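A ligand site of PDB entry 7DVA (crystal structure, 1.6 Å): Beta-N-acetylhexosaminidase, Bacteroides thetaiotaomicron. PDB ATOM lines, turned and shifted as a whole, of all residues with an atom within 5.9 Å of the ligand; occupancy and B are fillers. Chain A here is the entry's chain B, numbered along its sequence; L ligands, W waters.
OE2 of Glu 316 lies within hydrogen-bond range of O1 of the ligand. An oxygen (O5) of the ligand sits at hydrogen-bond distance from the side-chain hydroxyl (OH) of Tyr 415 (2.7 Å). OE2 of Glu 467 lies within hydrogen-bond range of O9 of the ligand (2.7 Å). O7 of the ligand lies within hydrogen-bond range of ND2 of Asn 417. An oxygen (O2) of the ligand is in hydrogen-bond range of the guanidinium group of Arg 151 (2.9 Å). OD2 of Asp 315 is in hydrogen-bond range of N1 of the ligand (2.9 Å). An oxygen (O8) of the ligand is in salt-bridge range of the guanidinium group (NH1) of Arg 418. An oxygen (O7) of the ligand sits close to the side-chain amide nitrogen (NE2) of Gln 430, at 3.4 Å. The side-chain amide nitrogen (NE2) of Gln 411 lies within hydrogen-bond range of an oxygen (O8) of the ligand (3.2 Å).
Glu 180 touches the ligand (OE2 to O2, 3.95 Å). CE1 of His 250 touches O2 of the ligand, at 3.5 Å. CD2 of Trp 369 touches C8 of the ligand, 3.5 Å away. Trp 389 touches the ligand (CH2 to C1, 3.4 Å). Trp 465 touches the ligand. Hydrophobic or aromatic side chains that line the ligand: His 250, Trp 369, Trp 389, Tyr 415 and Trp 465. 14 residues have an atom within 4 Å of the ligand: Arg 151, Glu 180, His 250, Asp 315, Glu 316, Trp 369, Trp 389, Gln 411, Tyr 415, Asn 417, Arg 418, Gln 430, Trp 465 and Glu 467. Along chain A the residues within 4 Å of the ligand span positions 151 to 467. The nearest printed residue that does not touch the ligand is Asp 148 (4.7 Å).
The side-chain carboxylate of Glu 316 is in hydrogen-bond range of a ring nitrogen (NE2) of His 250. The guanidinium group (NH1) of Arg 151 is in salt-bridge range of the side-chain carboxylate (OE2) of Glu 467. The side-chain amide nitrogen of Asn 417 sits at hydrogen-bond distance from the side-chain amide oxygen of Gln 430. The side-chain amide oxygen of Asn 417 sits at hydrogen-bond distance from the backbone NH of Trp 465 (3.0 Å). The guanidinium group of Arg 151 lies within salt-bridge range of the side-chain carboxylate of Asp 148 (2.9 Å). The side-chain carboxylate (OE1) of Glu 371 lies within hydrogen-bond range of the indole nitrogen (NE1) of Trp 389 (2.9 Å). ND1 of His 250 sits at hydrogen-bond distance from OE1 of Glu 180 (2.7 Å). The side-chain carboxylate of Glu 180 lies within hydrogen-bond range of a ring nitrogen (NE2) of His 177, at 2.6 Å.
Water W1 lies within hydrogen-bond range of O2 of the ligand (2.6 Å), OD2 of Asp 315 (2.7 Å), OE2 of Glu 180 (2.8 Å) and ND1 of His 250 (3.5 Å). Water W3 bridges OE1 of Glu 316 (2.8 Å) and O1 of the ligand (3.5 Å).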
ATOM      1  N   ASP A 148     -11.877 -26.377 -23.414  1.00  0.00           N
ATOM      2  CA  ASP A 148     -12.939 -25.430 -23.750  1.00  0.00           C
ATOM      3  C   ASP A 148     -14.221 -26.226 -23.984  1.00  0.00           C
ATOM      4  O   ASP A 148     -14.316 -26.944 -24.984  1.00  0.00           O
ATOM      5  CB  ASP A 148     -12.529 -24.706 -25.035  1.00  0.00           C
ATOM      6  CG  ASP A 148     -13.584 -23.900 -25.758  1.00  0.00           C
ATOM      7  OD1 ASP A 148     -14.665 -23.631 -25.159  1.00  0.00           O
ATOM      8  OD2 ASP A 148     -13.306 -23.522 -26.930  1.00  0.00           O
ATOM      9  N   ARG A 151     -17.381 -23.693 -26.485  1.00  0.00           N
ATOM     10  CA  ARG A 151     -17.614 -23.751 -27.913  1.00  0.00           C
ATOM     11  C   ARG A 151     -18.389 -25.022 -28.258  1.00  0.00           C
ATOM     12  O   ARG A 151     -19.435 -24.942 -28.897  1.00  0.00           O
ATOM     13  CB  ARG A 151     -16.302 -23.656 -28.704  1.00  0.00           C
ATOM     14  CG  ARG A 151     -15.843 -22.220 -28.929  1.00  0.00           C
ATOM     15  CD  ARG A 151     -15.684 -21.392 -27.655  1.00  0.00           C
ATOM     16  NE  ARG A 151     -15.120 -20.082 -27.925  1.00  0.00           N
ATOM     17  CZ  ARG A 151     -13.810 -19.829 -28.024  1.00  0.00           C
ATOM     18  NH1 ARG A 151     -12.949 -20.814 -27.859  1.00  0.00           N
ATOM     19  NH2 ARG A 151     -13.366 -18.606 -28.315  1.00  0.00           N
ATOM     20  N   HIS A 177     -12.571 -24.497 -19.001  1.00  0.00           N
ATOM     21  CA  HIS A 177     -13.010 -23.283 -19.660  1.00  0.00           C
ATOM     22  C   HIS A 177     -14.501 -23.438 -19.995  1.00  0.00           C
ATOM     23  O   HIS A 177     -14.852 -23.971 -21.056  1.00  0.00           O
ATOM     24  CB  HIS A 177     -12.095 -23.031 -20.884  1.00  0.00           C
ATOM     25  CG  HIS A 177     -12.353 -21.737 -21.578  1.00  0.00           C
ATOM     26  ND1 HIS A 177     -11.686 -20.579 -21.229  1.00  0.00           N
ATOM     27  CD2 HIS A 177     -13.153 -21.420 -22.619  1.00  0.00           C
ATOM     28  CE1 HIS A 177     -12.088 -19.596 -22.012  1.00  0.00           C
ATOM     29  NE2 HIS A 177     -12.988 -20.088 -22.865  1.00  0.00           N
ATOM     30  N   GLU A 180     -18.202 -18.826 -22.415  1.00  0.00           N
ATOM     31  CA  GLU A 180     -17.733 -18.280 -23.684  1.00  0.00           C
ATOM     32  C   GLU A 180     -18.805 -17.403 -24.316  1.00  0.00           C
ATOM     33  O   GLU A 180     -19.924 -17.277 -23.827  1.00  0.00           O
ATOM     34  CB  GLU A 180     -17.353 -19.415 -24.635  1.00  0.00           C
ATOM     35  CG  GLU A 180     -15.866 -19.711 -24.620  1.00  0.00           C
ATOM     36  CD  GLU A 180     -15.012 -18.527 -25.091  1.00  0.00           C
ATOM     37  OE1 GLU A 180     -15.579 -17.652 -25.791  1.00  0.00           O
ATOM     38  OE2 GLU A 180     -13.787 -18.480 -24.745  1.00  0.00           O
ATOM     39  N   HIS A 250     -15.246 -12.415 -23.872  1.00  0.00           N
ATOM     40  CA  HIS A 250     -15.665 -13.794 -24.092  1.00  0.00           C
ATOM     41  C   HIS A 250     -16.920 -14.119 -23.292  1.00  0.00           C
ATOM     42  O   HIS A 250     -17.072 -15.240 -22.816  1.00  0.00           O
ATOM     43  CB  HIS A 250     -14.488 -14.741 -23.793  1.00  0.00           C
ATOM     44  CG  HIS A 250     -13.521 -14.815 -24.928  1.00  0.00           C
ATOM     45  ND1 HIS A 250     -13.692 -15.700 -25.973  1.00  0.00           N
ATOM     46  CD2 HIS A 250     -12.433 -14.061 -25.223  1.00  0.00           C
ATOM     47  CE1 HIS A 250     -12.730 -15.529 -26.859  1.00  0.00           C
ATOM     48  NE2 HIS A 250     -11.937 -14.526 -26.417  1.00  0.00           N
ATOM     49  N   ILE A 278     -13.601 -12.977 -32.123  1.00  0.00           N
ATOM     50  CA  ILE A 278     -13.557 -12.058 -30.991  1.00  0.00           C
ATOM     51  C   ILE A 278     -14.815 -11.188 -31.011  1.00  0.00           C
ATOM     52  O   ILE A 278     -15.071 -10.484 -31.984  1.00  0.00           O
ATOM     53  CB  ILE A 278     -12.267 -11.212 -31.042  1.00  0.00           C
ATOM     54  CG1 ILE A 278     -11.024 -12.095 -30.953  1.00  0.00           C
ATOM     55  CG2 ILE A 278     -12.285 -10.132 -29.973  1.00  0.00           C
ATOM     56  CD1 ILE A 278      -9.715 -11.348 -31.150  1.00  0.00           C
ATOM     57  N   ASP A 315      -8.723 -12.527 -21.700  1.00  0.00           N
ATOM     58  CA  ASP A 315      -8.228 -12.489 -23.067  1.00  0.00           C
ATOM     59  C   ASP A 315      -9.189 -11.701 -23.962  1.00  0.00           C
ATOM     60  O   ASP A 315     -10.390 -11.615 -23.701  1.00  0.00           O
ATOM     61  CB  ASP A 315      -8.028 -13.909 -23.614  1.00  0.00           C
ATOM     62  CG  ASP A 315      -9.298 -14.745 -23.608  1.00  0.00           C
ATOM     63  OD1 ASP A 315     -10.061 -14.691 -22.608  1.00  0.00           O
ATOM     64  OD2 ASP A 315      -9.510 -15.446 -24.617  1.00  0.00           O
ATOM     65  N   GLU A 316      -8.635 -11.105 -25.032  1.00  0.00           N
ATOM     66  CA  GLU A 316      -9.405 -10.625 -26.181  1.00  0.00           C
ATOM     67  C   GLU A 316     -10.677  -9.893 -25.762  1.00  0.00           C
ATOM     68  O   GLU A 316     -11.780 -10.256 -26.168  1.00  0.00           O
ATOM     69  CB  GLU A 316      -9.775 -11.825 -27.056  1.00  0.00           C
ATOM     70  CG  GLU A 316      -8.545 -12.505 -27.611  1.00  0.00           C
ATOM     71  CD  GLU A 316      -8.826 -13.764 -28.402  1.00  0.00           C
ATOM     72  OE1 GLU A 316      -9.938 -14.346 -28.233  1.00  0.00           O
ATOM     73  OE2 GLU A 316      -7.954 -14.153 -29.205  1.00  0.00           O
ATOM     74  N   TRP A 369      -5.347 -14.622 -18.337  1.00  0.00           N
ATOM     75  CA  TRP A 369      -4.583 -14.670 -19.583  1.00  0.00           C
ATOM     76  C   TRP A 369      -3.678 -13.435 -19.664  1.00  0.00           C
ATOM     77  O   TRP A 369      -3.982 -12.400 -19.080  1.00  0.00           O
ATOM     78  CB  TRP A 369      -5.527 -14.749 -20.783  1.00  0.00           C
ATOM     79  CG  TRP A 369      -6.426 -15.952 -20.779  1.00  0.00           C
ATOM     80  CD1 TRP A 369      -7.783 -15.950 -20.602  1.00  0.00           C
ATOM     81  CD2 TRP A 369      -6.040 -17.314 -20.980  1.00  0.00           C
ATOM     82  NE1 TRP A 369      -8.271 -17.240 -20.671  1.00  0.00           N
ATOM     83  CE2 TRP A 369      -7.219 -18.094 -20.884  1.00  0.00           C
ATOM     84  CE3 TRP A 369      -4.807 -17.969 -21.201  1.00  0.00           C
ATOM     85  CZ2 TRP A 369      -7.210 -19.470 -21.056  1.00  0.00           C
ATOM     86  CZ3 TRP A 369      -4.794 -19.336 -21.355  1.00  0.00           C
ATOM     87  CH2 TRP A 369      -5.981 -20.080 -21.267  1.00  0.00           C
ATOM     88  N   GLU A 371      -3.087 -11.010 -21.669  1.00  0.00           N
ATOM     89  CA  GLU A 371      -3.446  -9.688 -22.184  1.00  0.00           C
ATOM     90  C   GLU A 371      -3.680  -8.703 -21.041  1.00  0.00           C
ATOM     91  O   GLU A 371      -3.575  -7.495 -21.253  1.00  0.00           O
ATOM     92  CB  GLU A 371      -4.722  -9.691 -23.030  1.00  0.00           C
ATOM     93  CG  GLU A 371      -4.539 -10.367 -24.367  1.00  0.00           C
ATOM     94  CD  GLU A 371      -5.040 -11.802 -24.389  1.00  0.00           C
ATOM     95  OE1 GLU A 371      -4.749 -12.559 -23.417  1.00  0.00           O
ATOM     96  OE2 GLU A 371      -5.742 -12.145 -25.376  1.00  0.00           O
ATOM     97  N   TRP A 389      -0.001 -17.182 -23.194  1.00  0.00           N
ATOM     98  CA  TRP A 389      -0.450 -17.982 -24.331  1.00  0.00           C
ATOM     99  C   TRP A 389      -0.101 -17.314 -25.665  1.00  0.00           C
ATOM    100  O   TRP A 389       0.159 -18.008 -26.626  1.00  0.00           O
ATOM    101  CB  TRP A 389      -1.962 -18.239 -24.233  1.00  0.00           C
ATOM    102  CG  TRP A 389      -2.808 -17.053 -24.583  1.00  0.00           C
ATOM    103  CD1 TRP A 389      -3.229 -16.054 -23.758  1.00  0.00           C
ATOM    104  CD2 TRP A 389      -3.371 -16.767 -25.877  1.00  0.00           C
ATOM    105  NE1 TRP A 389      -3.997 -15.150 -24.456  1.00  0.00           N
ATOM    106  CE2 TRP A 389      -4.101 -15.557 -25.765  1.00  0.00           C
ATOM    107  CE3 TRP A 389      -3.302 -17.383 -27.142  1.00  0.00           C
ATOM    108  CZ2 TRP A 389      -4.756 -14.967 -26.847  1.00  0.00           C
ATOM    109  CZ3 TRP A 389      -3.955 -16.805 -28.218  1.00  0.00           C
ATOM    110  CH2 TRP A 389      -4.658 -15.600 -28.074  1.00  0.00           C
ATOM    111  N   GLN A 411       0.343 -20.738 -27.504  1.00  0.00           N
ATOM    112  CA  GLN A 411      -0.508 -21.125 -28.622  1.00  0.00           C
ATOM    113  C   GLN A 411       0.211 -22.151 -29.507  1.00  0.00           C
ATOM    114  O   GLN A 411      -0.313 -23.233 -29.799  1.00  0.00           O
ATOM    115  CB  GLN A 411      -0.885 -19.883 -29.437  1.00  0.00           C
ATOM    116  CG  GLN A 411      -1.710 -20.228 -30.677  1.00  0.00           C
ATOM    117  CD  GLN A 411      -1.877 -19.009 -31.558  1.00  0.00           C
ATOM    118  OE1 GLN A 411      -0.909 -18.332 -31.900  1.00  0.00           O
ATOM    119  NE2 GLN A 411      -3.115 -18.722 -31.910  1.00  0.00           N
ATOM    120  N   ILE A 412       1.416 -21.779 -29.952  1.00  0.00           N
ATOM    121  CA  ILE A 412       2.287 -22.714 -30.663  1.00  0.00           C
ATOM    122  C   ILE A 412       3.410 -23.050 -29.702  1.00  0.00           C
ATOM    123  O   ILE A 412       4.141 -22.149 -29.306  1.00  0.00           O
ATOM    124  CB  ILE A 412       2.864 -22.072 -31.938  1.00  0.00           C
ATOM    125  CG1 ILE A 412       1.769 -21.456 -32.815  1.00  0.00           C
ATOM    126  CG2 ILE A 412       3.741 -23.060 -32.690  1.00  0.00           C
ATOM    127  CD1 ILE A 412       0.843 -22.460 -33.415  1.00  0.00           C
ATOM    128  N   TYR A 415      -1.220 -25.461 -27.941  1.00  0.00           N
ATOM    129  CA  TYR A 415      -2.652 -25.565 -28.235  1.00  0.00           C
ATOM    130  C   TYR A 415      -2.871 -26.848 -29.038  1.00  0.00           C
ATOM    131  O   TYR A 415      -2.722 -26.845 -30.255  1.00  0.00           O
ATOM    132  CB  TYR A 415      -3.122 -24.317 -28.976  1.00  0.00           C
ATOM    133  CG  TYR A 415      -3.399 -23.126 -28.089  1.00  0.00           C
ATOM    134  CD1 TYR A 415      -2.844 -23.032 -26.817  1.00  0.00           C
ATOM    135  CD2 TYR A 415      -4.213 -22.100 -28.519  1.00  0.00           C
ATOM    136  CE1 TYR A 415      -3.112 -21.957 -25.984  1.00  0.00           C
ATOM    137  CE2 TYR A 415      -4.491 -21.012 -27.703  1.00  0.00           C
ATOM    138  CZ  TYR A 415      -3.962 -20.959 -26.415  1.00  0.00           C
ATOM    139  OH  TYR A 415      -4.268 -19.934 -25.593  1.00  0.00           O
ATOM    140  N   ASN A 417      -5.388 -28.626 -29.727  1.00  0.00           N
ATOM    141  CA  ASN A 417      -6.491 -28.722 -30.674  1.00  0.00           C
ATOM    142  C   ASN A 417      -5.999 -28.514 -32.098  1.00  0.00           C
ATOM    143  O   ASN A 417      -6.704 -28.846 -33.033  1.00  0.00           O
ATOM    144  CB  ASN A 417      -7.624 -27.727 -30.406  1.00  0.00           C
ATOM    145  CG  ASN A 417      -7.119 -26.308 -30.295  1.00  0.00           C
ATOM    146  OD1 ASN A 417      -6.565 -25.937 -29.257  1.00  0.00           O
ATOM    147  ND2 ASN A 417      -7.268 -25.517 -31.350  1.00  0.00           N
ATOM    148  N   ARG A 418      -4.814 -27.906 -32.262  1.00  0.00           N
ATOM    149  CA  ARG A 418      -4.309 -27.576 -33.595  1.00  0.00           C
ATOM    150  C   ARG A 418      -3.897 -28.855 -34.310  1.00  0.00           C
ATOM    151  O   ARG A 418      -3.607 -29.862 -33.688  1.00  0.00           O
ATOM    152  CB  ARG A 418      -3.153 -26.574 -33.494  1.00  0.00           C
ATOM    153  CG  ARG A 418      -3.570 -25.196 -33.018  1.00  0.00           C
ATOM    154  CD  ARG A 418      -2.401 -24.259 -32.710  1.00  0.00           C
ATOM    155  NE  ARG A 418      -1.750 -23.920 -33.961  1.00  0.00           N
ATOM    156  CZ  ARG A 418      -2.007 -22.847 -34.708  1.00  0.00           C
ATOM    157  NH1 ARG A 418      -2.892 -21.944 -34.313  1.00  0.00           N
ATOM    158  NH2 ARG A 418      -1.353 -22.656 -35.832  1.00  0.00           N
ATOM    159  N   GLN A 430      -7.808 -25.918 -36.123  1.00  0.00           N
ATOM    160  CA  GLN A 430      -6.938 -24.786 -36.406  1.00  0.00           C
ATOM    161  C   GLN A 430      -5.541 -25.259 -36.785  1.00  0.00           C
ATOM    162  O   GLN A 430      -5.130 -26.357 -36.416  1.00  0.00           O
ATOM    163  CB  GLN A 430      -6.895 -23.834 -35.211  1.00  0.00           C
ATOM    164  CG  GLN A 430      -8.250 -23.211 -34.877  1.00  0.00           C
ATOM    165  CD  GLN A 430      -9.012 -23.940 -33.794  1.00  0.00           C
ATOM    166  OE1 GLN A 430      -8.911 -25.154 -33.633  1.00  0.00           O
ATOM    167  NE2 GLN A 430      -9.814 -23.185 -33.056  1.00  0.00           N
ATOM    168  N   GLY A 431      -4.799 -24.397 -37.508  1.00  0.00           N
ATOM    169  CA  GLY A 431      -3.429 -24.666 -37.889  1.00  0.00           C
ATOM    170  C   GLY A 431      -3.301 -25.474 -39.177  1.00  0.00           C
ATOM    171  O   GLY A 431      -4.300 -25.933 -39.737  1.00  0.00           O
ATOM    172  N   ASN A 463      -3.581 -26.564 -23.950  1.00  0.00           N
ATOM    173  CA  ASN A 463      -4.943 -26.065 -24.000  1.00  0.00           C
ATOM    174  C   ASN A 463      -5.623 -26.644 -25.222  1.00  0.00           C
ATOM    175  O   ASN A 463      -4.986 -26.863 -26.267  1.00  0.00           O
ATOM    176  CB  ASN A 463      -5.002 -24.528 -24.045  1.00  0.00           C
ATOM    177  CG  ASN A 463      -4.437 -23.834 -22.827  1.00  0.00           C
ATOM    178  OD1 ASN A 463      -4.212 -24.445 -21.795  1.00  0.00           O
ATOM    179  ND2 ASN A 463      -4.220 -22.522 -22.923  1.00  0.00           N
ATOM    180  N   TRP A 465      -8.978 -25.945 -27.495  1.00  0.00           N
ATOM    181  CA  TRP A 465     -10.064 -25.056 -27.875  1.00  0.00           C
ATOM    182  C   TRP A 465     -10.973 -25.776 -28.867  1.00  0.00           C
ATOM    183  O   TRP A 465     -10.473 -26.492 -29.749  1.00  0.00           O
ATOM    184  CB  TRP A 465      -9.489 -23.771 -28.482  1.00  0.00           C
ATOM    185  CG  TRP A 465      -8.590 -23.096 -27.498  1.00  0.00           C
ATOM    186  CD1 TRP A 465      -7.219 -23.159 -27.460  1.00  0.00           C
ATOM    187  CD2 TRP A 465      -8.991 -22.288 -26.386  1.00  0.00           C
ATOM    188  NE1 TRP A 465      -6.757 -22.426 -26.393  1.00  0.00           N
ATOM    189  CE2 TRP A 465      -7.809 -21.869 -25.738  1.00  0.00           C
ATOM    190  CE3 TRP A 465     -10.231 -21.849 -25.905  1.00  0.00           C
ATOM    191  CZ2 TRP A 465      -7.846 -21.034 -24.612  1.00  0.00           C
ATOM    192  CZ3 TRP A 465     -10.257 -21.036 -24.792  1.00  0.00           C
ATOM    193  CH2 TRP A 465      -9.085 -20.632 -24.157  1.00  0.00           C
ATOM    194  N   THR A 466     -12.293 -25.585 -28.732  1.00  0.00           N
ATOM    195  CA  THR A 466     -13.187 -26.502 -29.433  1.00  0.00           C
ATOM    196  C   THR A 466     -14.052 -25.821 -30.487  1.00  0.00           C
ATOM    197  O   THR A 466     -15.107 -26.362 -30.828  1.00  0.00           O
ATOM    198  CB  THR A 466     -14.019 -27.328 -28.444  1.00  0.00           C
ATOM    199  OG1 THR A 466     -14.782 -26.439 -27.626  1.00  0.00           O
ATOM    200  CG2 THR A 466     -13.162 -28.237 -27.588  1.00  0.00           C
ATOM    201  N   GLU A 467     -13.592 -24.719 -31.086  1.00  0.00           N
ATOM    202  CA  GLU A 467     -14.372 -24.098 -32.148  1.00  0.00           C
ATOM    203  C   GLU A 467     -14.772 -25.122 -33.217  1.00  0.00           C
ATOM    204  O   GLU A 467     -15.909 -25.086 -33.696  1.00  0.00           O
ATOM    205  CB  GLU A 467     -13.587 -23.039 -32.918  1.00  0.00           C
ATOM    206  CG  GLU A 467     -13.444 -21.714 -32.204  1.00  0.00           C
ATOM    207  CD  GLU A 467     -12.194 -21.629 -31.351  1.00  0.00           C
ATOM    208  OE1 GLU A 467     -11.710 -22.685 -30.870  1.00  0.00           O
ATOM    209  OE2 GLU A 467     -11.697 -20.499 -31.160  1.00  0.00           O
HETATM  210  C1  LIG L   1      -7.437 -17.455 -28.770  1.00  0.00           C
HETATM  211  C2  LIG L   1      -8.566 -17.476 -27.722  1.00  0.00           C
HETATM  212  C3  LIG L   1      -9.396 -18.770 -27.660  1.00  0.00           C
HETATM  213  C4  LIG L   1      -9.429 -19.467 -28.998  1.00  0.00           C
HETATM  214  C5  LIG L   1      -7.980 -19.841 -29.304  1.00  0.00           C
HETATM  215  C6  LIG L   1      -7.853 -20.619 -30.596  1.00  0.00           C
HETATM  216  O1  LIG L   1      -7.771 -16.515 -29.753  1.00  0.00           O
HETATM  217  O2  LIG L   1     -10.721 -18.420 -27.240  1.00  0.00           O
HETATM  218  O3  LIG L   1      -7.198 -18.654 -29.529  1.00  0.00           O
HETATM  219  O4  LIG L   1      -6.456 -20.859 -30.778  1.00  0.00           O
HETATM  220  N1  LIG L   1      -8.045 -17.162 -26.379  1.00  0.00           N
HETATM  221  C7  LIG L   1      -7.041 -17.855 -25.812  1.00  0.00           C
HETATM  222  O5  LIG L   1      -6.483 -18.738 -26.428  1.00  0.00           O
HETATM  223  C8  LIG L   1      -6.652 -17.491 -24.410  1.00  0.00           C
HETATM  224  S1  LIG L   1      -6.012 -21.543 -32.073  1.00  0.00           S
HETATM  225  O6  LIG L   1      -6.578 -20.700 -33.301  1.00  0.00           O
HETATM  226  O7  LIG L   1      -6.573 -22.851 -32.071  1.00  0.00           O
HETATM  227  O8  LIG L   1      -4.566 -21.596 -31.985  1.00  0.00           O
HETATM  228  O9  LIG L   1     -10.247 -20.630 -28.918  1.00  0.00           O
HETATM  229  O   HOH W   1     -11.122 -17.652 -24.736  1.00  0.00           O
HETATM  230  O   HOH W   2      -5.716 -20.216 -35.652  1.00  0.00           O
HETATM  231  O   HOH W   3     -11.153 -15.948 -30.195  1.00  0.00           O
